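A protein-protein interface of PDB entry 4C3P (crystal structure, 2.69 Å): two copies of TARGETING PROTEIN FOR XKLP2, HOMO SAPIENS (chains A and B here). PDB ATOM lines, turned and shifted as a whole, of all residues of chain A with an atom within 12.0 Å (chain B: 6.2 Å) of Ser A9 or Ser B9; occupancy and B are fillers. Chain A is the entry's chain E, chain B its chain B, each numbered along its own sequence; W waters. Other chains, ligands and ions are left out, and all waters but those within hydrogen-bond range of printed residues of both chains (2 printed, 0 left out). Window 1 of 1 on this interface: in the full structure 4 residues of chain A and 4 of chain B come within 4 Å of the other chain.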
ATOM      1  N   VAL A   4      -9.688 -33.046  19.135  1.00  0.00           N
ATOM      2  CA  VAL A   4      -9.352 -31.875  19.993  1.00  0.00           C
ATOM      3  C   VAL A   4     -10.546 -30.914  20.074  1.00  0.00           C
ATOM      4  O   VAL A   4     -10.942 -30.303  19.074  1.00  0.00           O
ATOM      5  CB  VAL A   4      -8.100 -31.113  19.465  1.00  0.00           C
ATOM      6  CG1 VAL A   4      -7.787 -29.891  20.321  1.00  0.00           C
ATOM      7  CG2 VAL A   4      -6.884 -32.032  19.411  1.00  0.00           C
ATOM      8  N   LYS A   5     -11.128 -30.816  21.267  1.00  0.00           N
ATOM      9  CA  LYS A   5     -11.947 -29.666  21.640  1.00  0.00           C
ATOM     10  C   LYS A   5     -11.012 -28.615  22.270  1.00  0.00           C
ATOM     11  O   LYS A   5      -9.794 -28.810  22.321  1.00  0.00           O
ATOM     12  CB  LYS A   5     -13.069 -30.077  22.602  1.00  0.00           C
ATOM     13  CG  LYS A   5     -12.609 -30.558  23.972  1.00  0.00           C
ATOM     14  CD  LYS A   5     -13.751 -30.564  24.979  1.00  0.00           C
ATOM     15  CE  LYS A   5     -14.788 -31.634  24.661  1.00  0.00           C
ATOM     16  NZ  LYS A   5     -15.899 -31.657  25.656  1.00  0.00           N
ATOM     17  N   SER A   6     -11.561 -27.499  22.741  1.00  0.00           N
ATOM     18  CA  SER A   6     -10.718 -26.450  23.311  1.00  0.00           C
ATOM     19  C   SER A   6     -10.559 -26.683  24.800  1.00  0.00           C
ATOM     20  O   SER A   6     -11.460 -27.182  25.469  1.00  0.00           O
ATOM     21  CB  SER A   6     -11.279 -25.054  23.020  1.00  0.00           C
ATOM     22  OG  SER A   6     -11.146 -24.722  21.638  1.00  0.00           O
ATOM     23  N   SER A   7      -9.384 -26.342  25.303  1.00  0.00           N
ATOM     24  CA  SER A   7      -9.063 -26.506  26.713  1.00  0.00           C
ATOM     25  C   SER A   7      -9.617 -25.336  27.500  1.00  0.00           C
ATOM     26  O   SER A   7      -9.790 -25.440  28.703  1.00  0.00           O
ATOM     27  CB  SER A   7      -7.551 -26.522  26.886  1.00  0.00           C
ATOM     28  OG  SER A   7      -6.991 -25.428  26.166  1.00  0.00           O
ATOM     29  N   TYR A   8      -9.842 -24.218  26.808  1.00  0.00           N
ATOM     30  CA  TYR A   8     -10.278 -22.969  27.409  1.00  0.00           C
ATOM     31  C   TYR A   8      -9.238 -22.381  28.370  1.00  0.00           C
ATOM     32  O   TYR A   8      -9.573 -21.729  29.363  1.00  0.00           O
ATOM     33  CB  TYR A   8     -11.667 -23.122  28.042  1.00  0.00           C
ATOM     34  CG  TYR A   8     -12.737 -23.396  26.983  1.00  0.00           C
ATOM     35  CD1 TYR A   8     -13.382 -22.342  26.324  1.00  0.00           C
ATOM     36  CD2 TYR A   8     -13.074 -24.701  26.616  1.00  0.00           C
ATOM     37  CE1 TYR A   8     -14.337 -22.583  25.343  1.00  0.00           C
ATOM     38  CE2 TYR A   8     -14.014 -24.945  25.641  1.00  0.00           C
ATOM     39  CZ  TYR A   8     -14.643 -23.884  25.010  1.00  0.00           C
ATOM     40  OH  TYR A   8     -15.578 -24.129  24.041  1.00  0.00           O
ATOM     41  N   SER A   9      -7.971 -22.610  28.063  1.00  0.00           N
ATOM     42  CA  SER A   9      -6.907 -22.014  28.834  1.00  0.00           C
ATOM     43  C   SER A   9      -6.620 -20.689  28.178  1.00  0.00           C
ATOM     44  O   SER A   9      -6.298 -20.643  27.013  1.00  0.00           O
ATOM     45  CB  SER A   9      -5.647 -22.877  28.815  1.00  0.00           C
ATOM     46  OG  SER A   9      -5.910 -24.146  29.383  1.00  0.00           O
ATOM     47  N   TYR A  10      -6.774 -19.605  28.923  1.00  0.00           N
ATOM     48  CA  TYR A  10      -6.454 -18.281  28.427  1.00  0.00           C
ATOM     49  C   TYR A  10      -5.324 -17.747  29.266  1.00  0.00           C
ATOM     50  O   TYR A  10      -5.120 -18.196  30.386  1.00  0.00           O
ATOM     51  CB  TYR A  10      -7.653 -17.356  28.543  1.00  0.00           C
ATOM     52  CG  TYR A  10      -8.881 -17.848  27.845  1.00  0.00           C
ATOM     53  CD1 TYR A  10      -8.818 -18.806  26.818  1.00  0.00           C
ATOM     54  CD2 TYR A  10     -10.117 -17.332  28.170  1.00  0.00           C
ATOM     55  CE1 TYR A  10      -9.966 -19.223  26.159  1.00  0.00           C
ATOM     56  CE2 TYR A  10     -11.269 -17.743  27.518  1.00  0.00           C
ATOM     57  CZ  TYR A  10     -11.185 -18.679  26.527  1.00  0.00           C
ATOM     58  OH  TYR A  10     -12.328 -19.060  25.911  1.00  0.00           O
ATOM     59  N   ASP A  11      -4.588 -16.804  28.700  1.00  0.00           N
ATOM     60  CA  ASP A  11      -3.604 -16.051  29.427  1.00  0.00           C
ATOM     61  C   ASP A  11      -4.362 -14.865  29.967  1.00  0.00           C
ATOM     62  O   ASP A  11      -4.251 -13.744  29.463  1.00  0.00           O
ATOM     63  CB  ASP A  11      -2.436 -15.627  28.509  1.00  0.00           C
ATOM     64  CG  ASP A  11      -1.629 -16.838  27.955  1.00  0.00           C
ATOM     65  OD1 ASP A  11      -1.344 -17.799  28.725  1.00  0.00           O
ATOM     66  OD2 ASP A  11      -1.262 -16.810  26.746  1.00  0.00           O
ATOM     67  N   ALA A  12      -5.148 -15.152  30.997  1.00  0.00           N
ATOM     68  CA  ALA A  12      -6.046 -14.190  31.647  1.00  0.00           C
ATOM     69  C   ALA A  12      -6.334 -14.615  33.105  1.00  0.00           C
ATOM     70  O   ALA A  12      -6.428 -15.815  33.407  1.00  0.00           O
ATOM     71  CB  ALA A  12      -7.346 -14.093  30.882  1.00  0.00           C
ATOM     72  N   PRO A  13      -6.495 -13.630  34.007  1.00  0.00           N
ATOM     73  CA  PRO A  13      -6.591 -13.974  35.401  1.00  0.00           C
ATOM     74  C   PRO A  13      -7.763 -14.901  35.674  1.00  0.00           C
ATOM     75  O   PRO A  13      -8.831 -14.738  35.082  1.00  0.00           O
ATOM     76  CB  PRO A  13      -6.798 -12.615  36.102  1.00  0.00           C
ATOM     77  CG  PRO A  13      -6.472 -11.564  35.103  1.00  0.00           C
ATOM     78  CD  PRO A  13      -6.774 -12.197  33.775  1.00  0.00           C
ATOM     79  N   SER A  14      -7.527 -15.869  36.560  1.00  0.00           N
ATOM     80  CA  SER A  14      -8.529 -16.822  37.007  1.00  0.00           C
ATOM     81  C   SER A  14      -8.470 -16.990  38.538  1.00  0.00           C
ATOM     82  O   SER A  14      -9.129 -17.877  39.110  1.00  0.00           O
ATOM     83  CB  SER A  14      -8.270 -18.170  36.319  1.00  0.00           C
ATOM     84  OG  SER A  14      -9.467 -18.908  36.126  1.00  0.00           O
ATOM     85  N   ASP A  15      -7.688 -16.131  39.195  1.00  0.00           N
ATOM     86  CA  ASP A  15      -7.450 -16.224  40.632  1.00  0.00           C
ATOM     87  C   ASP A  15      -8.593 -15.552  41.395  1.00  0.00           C
ATOM     88  O   ASP A  15      -9.092 -14.519  40.978  1.00  0.00           O
ATOM     89  CB  ASP A  15      -6.103 -15.563  40.997  1.00  0.00           C
ATOM     90  CG  ASP A  15      -4.887 -16.207  40.266  1.00  0.00           C
ATOM     91  OD1 ASP A  15      -4.748 -17.472  40.285  1.00  0.00           O
ATOM     92  OD2 ASP A  15      -4.068 -15.435  39.678  1.00  0.00           O
ATOM     93  N   SER B   7       1.103 -19.828  29.812  1.00  0.00           N
ATOM     94  CA  SER B   7       0.747 -21.228  30.152  1.00  0.00           C
ATOM     95  C   SER B   7       1.070 -22.296  29.074  1.00  0.00           C
ATOM     96  O   SER B   7       1.053 -23.509  29.350  1.00  0.00           O
ATOM     97  CB  SER B   7      -0.729 -21.331  30.504  1.00  0.00           C
ATOM     98  OG  SER B   7      -0.982 -22.585  31.112  1.00  0.00           O
ATOM     99  N   TYR B   8       1.321 -21.837  27.849  1.00  0.00           N
ATOM    100  CA  TYR B   8       1.701 -22.699  26.726  1.00  0.00           C
ATOM    101  C   TYR B   8       0.716 -23.836  26.443  1.00  0.00           C
ATOM    102  O   TYR B   8       1.128 -24.892  25.981  1.00  0.00           O
ATOM    103  CB  TYR B   8       3.147 -23.202  26.911  1.00  0.00           C
ATOM    104  CG  TYR B   8       4.129 -22.053  26.926  1.00  0.00           C
ATOM    105  CD1 TYR B   8       4.655 -21.548  25.753  1.00  0.00           C
ATOM    106  CD2 TYR B   8       4.481 -21.428  28.116  1.00  0.00           C
ATOM    107  CE1 TYR B   8       5.523 -20.475  25.768  1.00  0.00           C
ATOM    108  CE2 TYR B   8       5.359 -20.353  28.136  1.00  0.00           C
ATOM    109  CZ  TYR B   8       5.866 -19.881  26.966  1.00  0.00           C
ATOM    110  OH  TYR B   8       6.737 -18.815  26.995  1.00  0.00           O
ATOM    111  N   SER B   9      -0.575 -23.609  26.708  1.00  0.00           N
ATOM    112  CA  SER B   9      -1.652 -24.504  26.218  1.00  0.00           C
ATOM    113  C   SER B   9      -2.237 -24.034  24.890  1.00  0.00           C
ATOM    114  O   SER B   9      -2.900 -23.016  24.847  1.00  0.00           O
ATOM    115  CB  SER B   9      -2.755 -24.635  27.242  1.00  0.00           C
ATOM    116  OG  SER B   9      -2.210 -25.266  28.393  1.00  0.00           O
ATOM    117  N   TYR B  10      -1.956 -24.757  23.807  1.00  0.00           N
ATOM    118  CA  TYR B  10      -2.460 -24.389  22.505  1.00  0.00           C
ATOM    119  C   TYR B  10      -3.488 -25.410  22.173  1.00  0.00           C
ATOM    120  O   TYR B  10      -3.292 -26.574  22.446  1.00  0.00           O
ATOM    121  CB  TYR B  10      -1.390 -24.452  21.433  1.00  0.00           C
ATOM    122  CG  TYR B  10      -0.108 -23.714  21.734  1.00  0.00           C
ATOM    123  CD1 TYR B  10      -0.063 -22.649  22.634  1.00  0.00           C
ATOM    124  CD2 TYR B  10       1.066 -24.064  21.091  1.00  0.00           C
ATOM    125  CE1 TYR B  10       1.115 -21.969  22.889  1.00  0.00           C
ATOM    126  CE2 TYR B  10       2.252 -23.395  21.344  1.00  0.00           C
ATOM    127  CZ  TYR B  10       2.272 -22.344  22.232  1.00  0.00           C
ATOM    128  OH  TYR B  10       3.465 -21.700  22.463  1.00  0.00           O
ATOM    129  N   ASP B  11      -4.584 -24.986  21.572  1.00  0.00           N
ATOM    130  CA  ASP B  11      -5.552 -25.912  21.015  1.00  0.00           C
ATOM    131  C   ASP B  11      -4.889 -26.577  19.823  1.00  0.00           C
ATOM    132  O   ASP B  11      -5.309 -26.382  18.676  1.00  0.00           O
ATOM    133  CB  ASP B  11      -6.823 -25.173  20.583  1.00  0.00           C
ATOM    134  CG  ASP B  11      -7.521 -24.469  21.743  1.00  0.00           C
ATOM    135  OD1 ASP B  11      -7.365 -24.923  22.904  1.00  0.00           O
ATOM    136  OD2 ASP B  11      -8.233 -23.461  21.483  1.00  0.00           O
ATOM    137  N   ALA B  12      -3.831 -27.341  20.110  1.00  0.00           N
ATOM    138  CA  ALA B  12      -3.082 -28.083  19.094  1.00  0.00           C
ATOM    139  C   ALA B  12      -2.663 -29.457  19.647  1.00  0.00           C
ATOM    140  O   ALA B  12      -2.593 -29.632  20.839  1.00  0.00           O
ATOM    141  CB  ALA B  12      -1.876 -27.276  18.660  1.00  0.00           C
HETATM  142  O   HOH W   1     -10.239 -23.809  19.087  1.00  0.00           O
HETATM  143  O   HOH W   2      -7.510 -21.889  24.387  1.00  0.00           O
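Ser A7 touches Asp B11, and with the chains exchanged Asp A11 touches Ser B7. Ser B9 touches its own counterpart, Ser A9. 6 positions are printed for both chains. Of the 4 pairs that touch across the chains among the printed residues, 3 have their exchanged pair printed and touching as well.
Of the 6 printed residues of chain B, 3 touch a printed residue of chain A. Among the printed residues, 4 pairs touch across the chains.
Water W1 lies within hydrogen-bond range of OG of Ser A6 (2.9 Å) and OD2 of Asp B11 (3.1 Å). Water W2 lies within hydrogen-bond range of O of Ser A9 (3.1 Å) and OD2 of Asp B11 (3.4 Å).
OD1 of Asp A11 is in hydrogen-bond range of N of Ser B7 (3.4 Å). OD2 of Asp B11 sits at hydrogen-bond distance from OG of Ser A6 (3.2 Å). The side-chain carboxylate (OD1) of Asp B11 is in hydrogen-bond range of the side-chain hydroxyl (OG) of Ser A7.
CB of Ser A9 touches CB of Ser B9, at 3.7 Å.
Of the printed residues of chain B, Ser A6 touches Asp B11. Printed residues of chain B within 4 Å of Ser A7: Asp B11 (3.3 Å). Of the printed residues of chain B, Asp A11 touches Ser B7 (3.4 Å). Pro A13 touches none of the printed residues of chain B. Ser B7 touches just one residue of chain A: Asp A11 (3.4 Å). Ser B9 touches just one residue of chain A: Ser A9. No residue of chain A comes within 4 Å of Tyr B10. The nearest residue of chain B that does not touch Ser A9 is Ser B7 (5.2 Å). The nearest residue of chain A that does not touch Ser B9 is Ser A7 (4.4 Å).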
